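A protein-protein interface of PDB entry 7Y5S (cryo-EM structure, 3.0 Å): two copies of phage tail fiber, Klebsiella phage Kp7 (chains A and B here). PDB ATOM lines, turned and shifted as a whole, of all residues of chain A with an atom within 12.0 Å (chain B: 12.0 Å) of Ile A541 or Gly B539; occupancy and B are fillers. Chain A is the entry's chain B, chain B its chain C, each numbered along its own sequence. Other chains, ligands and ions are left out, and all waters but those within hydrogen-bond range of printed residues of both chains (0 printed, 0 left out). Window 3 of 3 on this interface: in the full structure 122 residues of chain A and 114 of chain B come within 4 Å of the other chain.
Of the printed residues of chain B, Thr A533 touches Ile B524. Of the printed residues of chain B, Ala A536 touches Val B531 and Gly B532. No residue of chain B comes within 4 Å of Gly A539. Of chain B, only Val B534, Ala B536 and Gly B539 come within 4 Å of Ile A541. Asn A542 touches three residues of chain B. Of the printed residues of chain A, Ile B524 touches Thr A533, Val A534 and Phe A535. Val B534 touches two residues of chain A. Of chain A, only Ile A541 and Asn A542 come within 4 Å of Ala B536. No residue of chain A comes within 4 Å of Ala B537. Printed residues of chain A within 4 Å of Gly B539: Ile A541. The nearest residue of chain B that does not touch Ile A541 is Thr B540 (4.5 Å).
Printed residues of chain B that touch a printed residue of chain A: Ile B524, Val B531, Gly B532, Thr B533, Val B534, Phe B535, Ala B536 and Gly B539. Hydrophobic or aromatic side chains of chain B that line the printed part of chain A: Ile B524, Val B531, Val B534, Phe B535 and Ala B536. Among the printed residues, 16 pairs touch across the chains. Among the printed residues, no Asp or Glu carboxylate lies within 4 Å of a Lys or Arg side-chain nitrogen of the other chain.
N of Val B531 is in hydrogen-bond range of O of Phe A535, at 3.2 Å. The backbone NH of Ala A537 is in hydrogen-bond range of the backbone carbonyl oxygen of Val B531 (3.0 Å). O of Thr A533 sits at hydrogen-bond distance from N of Ile B524 (2.9 Å). O of Val B534 is in hydrogen-bond range of N of Asn A542. N of Phe A535 lies within hydrogen-bond range of O of Ile B524 (2.9 Å). The side-chain amide nitrogen of Asn A542 sits at hydrogen-bond distance from the backbone carbonyl oxygen of Ala B536.
Among the printed residues, merely in contact across the chains: Thr A538 with Thr B533 (3.2 Å), Val A534 with Ile B524 (3.3 Å), Ala A536 with Val B531 (3.3 Å), Ala A536 with Gly B532 (3.3 Å), Asn A542 with Phe B535 (3.4 Å), Ile A541 with Ala B536 (3.4 Å), Ile A541 with Gly B539 (3.6 Å), Ala A537 with Gly B532 (3.6 Å), Ile A541 with Val B534 (3.6 Å) and Thr A538 with Gly B532 (3.7 Å).
Phe A535 touches Ile B524, but with the chains exchanged Ile A524 does not touch Phe B535 (7.4 Å). Ala A536 touches Gly B532, but with the chains exchanged Gly A532 does not touch Ala B536 (13.8 Å). Ala A537 touches Val B531, but with the chains exchanged Val A531 does not touch Ala B537 (14.3 Å). Asn A542 touches Val B534, but with the chains exchanged Val A534 does not touch Asn B542 (9.5 Å). 13 positions are printed for both chains.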
ATOM      1  N   ILE A 514      -8.546   9.201 -30.124  1.00  0.00           N
ATOM      2  CA  ILE A 514      -8.578  10.648 -30.302  1.00  0.00           C
ATOM      3  C   ILE A 514      -7.130  11.120 -30.244  1.00  0.00           C
ATOM      4  O   ILE A 514      -6.526  11.174 -29.169  1.00  0.00           O
ATOM      5  CB  ILE A 514      -9.438  11.333 -29.238  1.00  0.00           C
ATOM      6  CG1 ILE A 514     -10.907  10.950 -29.412  1.00  0.00           C
ATOM      7  CG2 ILE A 514      -9.279  12.845 -29.314  1.00  0.00           C
ATOM      8  CD1 ILE A 514     -11.796  11.425 -28.288  1.00  0.00           C
ATOM      9  N   ASP A 519       2.573  16.786 -32.263  1.00  0.00           N
ATOM     10  CA  ASP A 519       2.986  16.087 -31.053  1.00  0.00           C
ATOM     11  C   ASP A 519       3.176  17.073 -29.906  1.00  0.00           C
ATOM     12  O   ASP A 519       3.993  17.996 -29.999  1.00  0.00           O
ATOM     13  CB  ASP A 519       4.277  15.310 -31.308  1.00  0.00           C
ATOM     14  CG  ASP A 519       4.616  14.350 -30.182  1.00  0.00           C
ATOM     15  OD1 ASP A 519       3.834  14.257 -29.212  1.00  0.00           O
ATOM     16  OD2 ASP A 519       5.673  13.688 -30.265  1.00  0.00           O
ATOM     17  N   GLY A 520       2.421  16.872 -28.826  1.00  0.00           N
ATOM     18  CA  GLY A 520       2.687  17.546 -27.570  1.00  0.00           C
ATOM     19  C   GLY A 520       2.490  19.043 -27.551  1.00  0.00           C
ATOM     20  O   GLY A 520       3.217  19.736 -26.833  1.00  0.00           O
ATOM     21  N   ILE A 521       1.536  19.573 -28.313  1.00  0.00           N
ATOM     22  CA  ILE A 521       1.255  21.004 -28.274  1.00  0.00           C
ATOM     23  C   ILE A 521      -0.216  21.226 -27.950  1.00  0.00           C
ATOM     24  O   ILE A 521      -0.609  22.309 -27.504  1.00  0.00           O
ATOM     25  CB  ILE A 521       1.636  21.696 -29.596  1.00  0.00           C
ATOM     26  CG1 ILE A 521       0.826  21.123 -30.760  1.00  0.00           C
ATOM     27  CG2 ILE A 521       3.127  21.553 -29.862  1.00  0.00           C
ATOM     28  CD1 ILE A 521       0.948  21.932 -32.030  1.00  0.00           C
ATOM     29  N   LYS A 522      -1.037  20.204 -28.174  1.00  0.00           N
ATOM     30  CA  LYS A 522      -2.474  20.315 -27.972  1.00  0.00           C
ATOM     31  C   LYS A 522      -2.866  19.741 -26.617  1.00  0.00           C
ATOM     32  O   LYS A 522      -2.403  18.666 -26.225  1.00  0.00           O
ATOM     33  CB  LYS A 522      -3.228  19.599 -29.093  1.00  0.00           C
ATOM     34  CG  LYS A 522      -2.858  20.112 -30.470  1.00  0.00           C
ATOM     35  CD  LYS A 522      -3.192  21.588 -30.598  1.00  0.00           C
ATOM     36  CE  LYS A 522      -2.936  22.098 -32.003  1.00  0.00           C
ATOM     37  NZ  LYS A 522      -2.113  23.337 -32.003  1.00  0.00           N
ATOM     38  N   ASN A 523      -3.726  20.466 -25.908  1.00  0.00           N
ATOM     39  CA  ASN A 523      -4.105  20.137 -24.545  1.00  0.00           C
ATOM     40  C   ASN A 523      -5.528  19.594 -24.495  1.00  0.00           C
ATOM     41  O   ASN A 523      -6.345  19.836 -25.387  1.00  0.00           O
ATOM     42  CB  ASN A 523      -3.986  21.366 -23.637  1.00  0.00           C
ATOM     43  CG  ASN A 523      -2.594  21.962 -23.642  1.00  0.00           C
ATOM     44  OD1 ASN A 523      -1.634  21.329 -23.200  1.00  0.00           O
ATOM     45  ND2 ASN A 523      -2.476  23.187 -24.141  1.00  0.00           N
ATOM     46  N   ILE A 524      -5.811  18.851 -23.429  1.00  0.00           N
ATOM     47  CA  ILE A 524      -7.150  18.363 -23.129  1.00  0.00           C
ATOM     48  C   ILE A 524      -7.652  19.177 -21.944  1.00  0.00           C
ATOM     49  O   ILE A 524      -7.209  18.979 -20.806  1.00  0.00           O
ATOM     50  CB  ILE A 524      -7.164  16.859 -22.829  1.00  0.00           C
ATOM     51  CG1 ILE A 524      -6.831  16.060 -24.090  1.00  0.00           C
ATOM     52  CG2 ILE A 524      -8.519  16.437 -22.278  1.00  0.00           C
ATOM     53  CD1 ILE A 524      -7.900  16.131 -25.157  1.00  0.00           C
ATOM     54  N   GLY A 525      -8.567  20.099 -22.201  1.00  0.00           N
ATOM     55  CA  GLY A 525      -9.044  21.006 -21.179  1.00  0.00           C
ATOM     56  C   GLY A 525      -8.262  22.303 -21.160  1.00  0.00           C
ATOM     57  O   GLY A 525      -7.335  22.530 -21.942  1.00  0.00           O
ATOM     58  N   VAL A 531     -12.084  19.923 -17.573  1.00  0.00           N
ATOM     59  CA  VAL A 531     -12.891  18.708 -17.651  1.00  0.00           C
ATOM     60  C   VAL A 531     -13.033  18.145 -16.243  1.00  0.00           C
ATOM     61  O   VAL A 531     -12.358  18.599 -15.312  1.00  0.00           O
ATOM     62  CB  VAL A 531     -12.276  17.671 -18.607  1.00  0.00           C
ATOM     63  CG1 VAL A 531     -12.021  18.291 -19.974  1.00  0.00           C
ATOM     64  CG2 VAL A 531     -10.998  17.093 -18.023  1.00  0.00           C
ATOM     65  N   GLY A 532     -13.905  17.156 -16.075  1.00  0.00           N
ATOM     66  CA  GLY A 532     -14.152  16.603 -14.759  1.00  0.00           C
ATOM     67  C   GLY A 532     -13.312  15.383 -14.448  1.00  0.00           C
ATOM     68  O   GLY A 532     -12.105  15.501 -14.212  1.00  0.00           O
ATOM     69  N   THR A 533     -13.929  14.205 -14.445  1.00  0.00           N
ATOM     70  CA  THR A 533     -13.251  12.965 -14.102  1.00  0.00           C
ATOM     71  C   THR A 533     -12.834  12.234 -15.372  1.00  0.00           C
ATOM     72  O   THR A 533     -13.607  12.144 -16.331  1.00  0.00           O
ATOM     73  CB  THR A 533     -14.151  12.059 -13.256  1.00  0.00           C
ATOM     74  OG1 THR A 533     -14.714  12.815 -12.178  1.00  0.00           O
ATOM     75  CG2 THR A 533     -13.350  10.901 -12.682  1.00  0.00           C
ATOM     76  N   VAL A 534     -11.611  11.713 -15.373  1.00  0.00           N
ATOM     77  CA  VAL A 534     -11.085  10.942 -16.495  1.00  0.00           C
ATOM     78  C   VAL A 534     -11.046   9.478 -16.082  1.00  0.00           C
ATOM     79  O   VAL A 534     -10.306   9.104 -15.164  1.00  0.00           O
ATOM     80  CB  VAL A 534      -9.694  11.439 -16.916  1.00  0.00           C
ATOM     81  CG1 VAL A 534      -9.035  10.441 -17.856  1.00  0.00           C
ATOM     82  CG2 VAL A 534      -9.796  12.810 -17.570  1.00  0.00           C
ATOM     83  N   PHE A 535     -11.846   8.651 -16.752  1.00  0.00           N
ATOM     84  CA  PHE A 535     -11.937   7.226 -16.453  1.00  0.00           C
ATOM     85  C   PHE A 535     -11.109   6.461 -17.479  1.00  0.00           C
ATOM     86  O   PHE A 535     -11.500   6.352 -18.646  1.00  0.00           O
ATOM     87  CB  PHE A 535     -13.393   6.761 -16.469  1.00  0.00           C
ATOM     88  CG  PHE A 535     -14.230   7.350 -15.371  1.00  0.00           C
ATOM     89  CD1 PHE A 535     -14.115   6.889 -14.070  1.00  0.00           C
ATOM     90  CD2 PHE A 535     -15.139   8.362 -15.640  1.00  0.00           C
ATOM     91  CE1 PHE A 535     -14.889   7.428 -13.058  1.00  0.00           C
ATOM     92  CE2 PHE A 535     -15.913   8.903 -14.632  1.00  0.00           C
ATOM     93  CZ  PHE A 535     -15.788   8.436 -13.340  1.00  0.00           C
ATOM     94  N   ALA A 536      -9.972   5.923 -17.043  1.00  0.00           N
ATOM     95  CA  ALA A 536      -9.073   5.184 -17.913  1.00  0.00           C
ATOM     96  C   ALA A 536      -8.711   3.856 -17.269  1.00  0.00           C
ATOM     97  O   ALA A 536      -8.666   3.732 -16.040  1.00  0.00           O
ATOM     98  CB  ALA A 536      -7.798   5.983 -18.217  1.00  0.00           C
ATOM     99  N   ALA A 537      -8.454   2.855 -18.116  1.00  0.00           N
ATOM    100  CA  ALA A 537      -8.150   1.520 -17.616  1.00  0.00           C
ATOM    101  C   ALA A 537      -6.745   1.430 -17.034  1.00  0.00           C
ATOM    102  O   ALA A 537      -6.509   0.641 -16.113  1.00  0.00           O
ATOM    103  CB  ALA A 537      -8.327   0.490 -18.732  1.00  0.00           C
ATOM    104  N   THR A 538      -5.803   2.220 -17.551  1.00  0.00           N
ATOM    105  CA  THR A 538      -4.418   2.111 -17.105  1.00  0.00           C
ATOM    106  C   THR A 538      -4.216   2.793 -15.756  1.00  0.00           C
ATOM    107  O   THR A 538      -3.817   2.155 -14.776  1.00  0.00           O
ATOM    108  CB  THR A 538      -3.480   2.706 -18.157  1.00  0.00           C
ATOM    109  OG1 THR A 538      -3.703   4.118 -18.256  1.00  0.00           O
ATOM    110  CG2 THR A 538      -3.729   2.062 -19.511  1.00  0.00           C
ATOM    111  N   GLY A 539      -4.485   4.092 -15.689  1.00  0.00           N
ATOM    112  CA  GLY A 539      -4.318   4.843 -14.464  1.00  0.00           C
ATOM    113  C   GLY A 539      -3.017   5.604 -14.336  1.00  0.00           C
ATOM    114  O   GLY A 539      -2.717   6.096 -13.242  1.00  0.00           O
ATOM    115  N   THR A 540      -2.239   5.718 -15.408  1.00  0.00           N
ATOM    116  CA  THR A 540      -0.965   6.420 -15.360  1.00  0.00           C
ATOM    117  C   THR A 540      -0.665   6.974 -16.743  1.00  0.00           C
ATOM    118  O   THR A 540      -0.849   6.282 -17.748  1.00  0.00           O
ATOM    119  CB  THR A 540       0.166   5.492 -14.894  1.00  0.00           C
ATOM    120  OG1 THR A 540      -0.078   5.079 -13.544  1.00  0.00           O
ATOM    121  CG2 THR A 540       1.512   6.200 -14.963  1.00  0.00           C
ATOM    122  N   ILE A 541      -0.208   8.228 -16.787  1.00  0.00           N
ATOM    123  CA  ILE A 541       0.137   8.848 -18.058  1.00  0.00           C
ATOM    124  C   ILE A 541       1.328   8.116 -18.673  1.00  0.00           C
ATOM    125  O   ILE A 541       2.197   7.589 -17.964  1.00  0.00           O
ATOM    126  CB  ILE A 541       0.437  10.343 -17.859  1.00  0.00           C
ATOM    127  CG1 ILE A 541      -0.775  11.055 -17.256  1.00  0.00           C
ATOM    128  CG2 ILE A 541       0.804  11.009 -19.178  1.00  0.00           C
ATOM    129  CD1 ILE A 541      -2.013  10.995 -18.120  1.00  0.00           C
ATOM    130  N   ASN A 542       1.358   8.069 -20.004  1.00  0.00           N
ATOM    131  CA  ASN A 542       2.435   7.432 -20.763  1.00  0.00           C
ATOM    132  C   ASN A 542       2.538   5.945 -20.441  1.00  0.00           C
ATOM    133  O   ASN A 542       2.312   5.098 -21.304  1.00  0.00           O
ATOM    134  CB  ASN A 542       3.777   8.122 -20.487  1.00  0.00           C
ATOM    135  CG  ASN A 542       3.940   9.413 -21.266  1.00  0.00           C
ATOM    136  OD1 ASN A 542       3.558   9.501 -22.431  1.00  0.00           O
ATOM    137  ND2 ASN A 542       4.511  10.423 -20.621  1.00  0.00           N
ATOM    138  N   ILE B 524     -14.261  12.771 -19.125  1.00  0.00           N
ATOM    139  CA  ILE B 524     -13.631  12.049 -20.223  1.00  0.00           C
ATOM    140  C   ILE B 524     -13.717  10.569 -19.873  1.00  0.00           C
ATOM    141  O   ILE B 524     -12.992  10.082 -18.998  1.00  0.00           O
ATOM    142  CB  ILE B 524     -12.183  12.493 -20.454  1.00  0.00           C
ATOM    143  CG1 ILE B 524     -12.142  13.929 -20.977  1.00  0.00           C
ATOM    144  CG2 ILE B 524     -11.484  11.555 -21.428  1.00  0.00           C
ATOM    145  CD1 ILE B 524     -12.696  14.084 -22.375  1.00  0.00           C
ATOM    146  N   VAL B 531     -11.977   4.718 -21.300  1.00  0.00           N
ATOM    147  CA  VAL B 531     -10.935   4.875 -22.311  1.00  0.00           C
ATOM    148  C   VAL B 531      -9.734   4.042 -21.883  1.00  0.00           C
ATOM    149  O   VAL B 531      -9.685   3.538 -20.755  1.00  0.00           O
ATOM    150  CB  VAL B 531     -10.548   6.352 -22.507  1.00  0.00           C
ATOM    151  CG1 VAL B 531     -11.781   7.193 -22.805  1.00  0.00           C
ATOM    152  CG2 VAL B 531      -9.807   6.880 -21.290  1.00  0.00           C
ATOM    153  N   GLY B 532      -8.760   3.889 -22.775  1.00  0.00           N
ATOM    154  CA  GLY B 532      -7.611   3.058 -22.480  1.00  0.00           C
ATOM    155  C   GLY B 532      -6.436   3.831 -21.917  1.00  0.00           C
ATOM    156  O   GLY B 532      -6.469   4.261 -20.760  1.00  0.00           O
ATOM    157  N   THR B 533      -5.393   4.017 -22.719  1.00  0.00           N
ATOM    158  CA  THR B 533      -4.177   4.689 -22.284  1.00  0.00           C
ATOM    159  C   THR B 533      -4.202   6.144 -22.725  1.00  0.00           C
ATOM    160  O   THR B 533      -4.576   6.453 -23.861  1.00  0.00           O
ATOM    161  CB  THR B 533      -2.933   3.997 -22.849  1.00  0.00           C
ATOM    162  OG1 THR B 533      -3.018   2.586 -22.618  1.00  0.00           O
ATOM    163  CG2 THR B 533      -1.677   4.533 -22.179  1.00  0.00           C
ATOM    164  N   VAL B 534      -3.804   7.038 -21.825  1.00  0.00           N
ATOM    165  CA  VAL B 534      -3.726   8.465 -22.113  1.00  0.00           C
ATOM    166  C   VAL B 534      -2.255   8.839 -22.235  1.00  0.00           C
ATOM    167  O   VAL B 534      -1.500   8.749 -21.258  1.00  0.00           O
ATOM    168  CB  VAL B 534      -4.425   9.298 -21.028  1.00  0.00           C
ATOM    169  CG1 VAL B 534      -4.063  10.769 -21.170  1.00  0.00           C
ATOM    170  CG2 VAL B 534      -5.931   9.104 -21.099  1.00  0.00           C
ATOM    171  N   PHE B 535      -1.845   9.253 -23.431  1.00  0.00           N
ATOM    172  CA  PHE B 535      -0.461   9.621 -23.710  1.00  0.00           C
ATOM    173  C   PHE B 535      -0.352  11.143 -23.694  1.00  0.00           C
ATOM    174  O   PHE B 535      -0.828  11.813 -24.616  1.00  0.00           O
ATOM    175  CB  PHE B 535      -0.008   9.053 -25.053  1.00  0.00           C
ATOM    176  CG  PHE B 535       0.072   7.555 -25.082  1.00  0.00           C
ATOM    177  CD1 PHE B 535       1.119   6.890 -24.467  1.00  0.00           C
ATOM    178  CD2 PHE B 535      -0.900   6.807 -25.731  1.00  0.00           C
ATOM    179  CE1 PHE B 535       1.194   5.509 -24.495  1.00  0.00           C
ATOM    180  CE2 PHE B 535      -0.828   5.429 -25.762  1.00  0.00           C
ATOM    181  CZ  PHE B 535       0.221   4.779 -25.145  1.00  0.00           C
ATOM    182  N   ALA B 536       0.284  11.682 -22.658  1.00  0.00           N
ATOM    183  CA  ALA B 536       0.447  13.119 -22.503  1.00  0.00           C
ATOM    184  C   ALA B 536       1.904  13.441 -22.209  1.00  0.00           C
ATOM    185  O   ALA B 536       2.627  12.642 -21.605  1.00  0.00           O
ATOM    186  CB  ALA B 536      -0.448  13.670 -21.385  1.00  0.00           C
ATOM    187  N   ALA B 537       2.329  14.631 -22.645  1.00  0.00           N
ATOM    188  CA  ALA B 537       3.722  15.028 -22.472  1.00  0.00           C
ATOM    189  C   ALA B 537       4.034  15.410 -21.031  1.00  0.00           C
ATOM    190  O   ALA B 537       5.169  15.228 -20.577  1.00  0.00           O
ATOM    191  CB  ALA B 537       4.056  16.188 -23.409  1.00  0.00           C
ATOM    192  N   THR B 538       3.053  15.940 -20.298  1.00  0.00           N
ATOM    193  CA  THR B 538       3.315  16.416 -18.943  1.00  0.00           C
ATOM    194  C   THR B 538       3.395  15.259 -17.954  1.00  0.00           C
ATOM    195  O   THR B 538       4.423  15.055 -17.299  1.00  0.00           O
ATOM    196  CB  THR B 538       2.232  17.413 -18.521  1.00  0.00           C
ATOM    197  OG1 THR B 538       0.972  16.736 -18.414  1.00  0.00           O
ATOM    198  CG2 THR B 538       2.117  18.532 -19.542  1.00  0.00           C
ATOM    199  N   GLY B 539       2.319  14.489 -17.834  1.00  0.00           N
ATOM    200  CA  GLY B 539       2.279  13.371 -16.917  1.00  0.00           C
ATOM    201  C   GLY B 539       1.634  13.645 -15.577  1.00  0.00           C
ATOM    202  O   GLY B 539       1.747  12.805 -14.676  1.00  0.00           O
ATOM    203  N   THR B 540       0.963  14.781 -15.416  1.00  0.00           N
ATOM    204  CA  THR B 540       0.329  15.124 -14.152  1.00  0.00           C
ATOM    205  C   THR B 540      -0.858  16.030 -14.435  1.00  0.00           C
ATOM    206  O   THR B 540      -0.758  16.957 -15.245  1.00  0.00           O
ATOM    207  CB  THR B 540       1.317  15.812 -13.200  1.00  0.00           C
ATOM    208  OG1 THR B 540       2.364  14.898 -12.852  1.00  0.00           O
ATOM    209  CG2 THR B 540       0.616  16.274 -11.929  1.00  0.00           C
ATOM    210  N   ILE B 541      -1.981  15.753 -13.769  1.00  0.00           N
ATOM    211  CA  ILE B 541      -3.170  16.573 -13.945  1.00  0.00           C
ATOM    212  C   ILE B 541      -2.896  17.980 -13.419  1.00  0.00           C
ATOM    213  O   ILE B 541      -2.121  18.177 -12.473  1.00  0.00           O
ATOM    214  CB  ILE B 541      -4.373  15.930 -13.234  1.00  0.00           C
ATOM    215  CG1 ILE B 541      -4.633  14.529 -13.788  1.00  0.00           C
ATOM    216  CG2 ILE B 541      -5.626  16.777 -13.404  1.00  0.00           C
ATOM    217  CD1 ILE B 541      -4.964  14.506 -15.262  1.00  0.00           C
ATOM    218  N   ASN B 542      -3.527  18.970 -14.050  1.00  0.00           N
ATOM    219  CA  ASN B 542      -3.404  20.376 -13.666  1.00  0.00           C
ATOM    220  C   ASN B 542      -1.963  20.861 -13.785  1.00  0.00           C
ATOM    221  O   ASN B 542      -1.657  21.732 -14.597  1.00  0.00           O
ATOM    222  CB  ASN B 542      -3.917  20.599 -12.238  1.00  0.00           C
ATOM    223  CG  ASN B 542      -5.430  20.673 -12.166  1.00  0.00           C
ATOM    224  OD1 ASN B 542      -6.077  21.261 -13.031  1.00  0.00           O
ATOM    225  ND2 ASN B 542      -6.000  20.071 -11.129  1.00  0.00           N
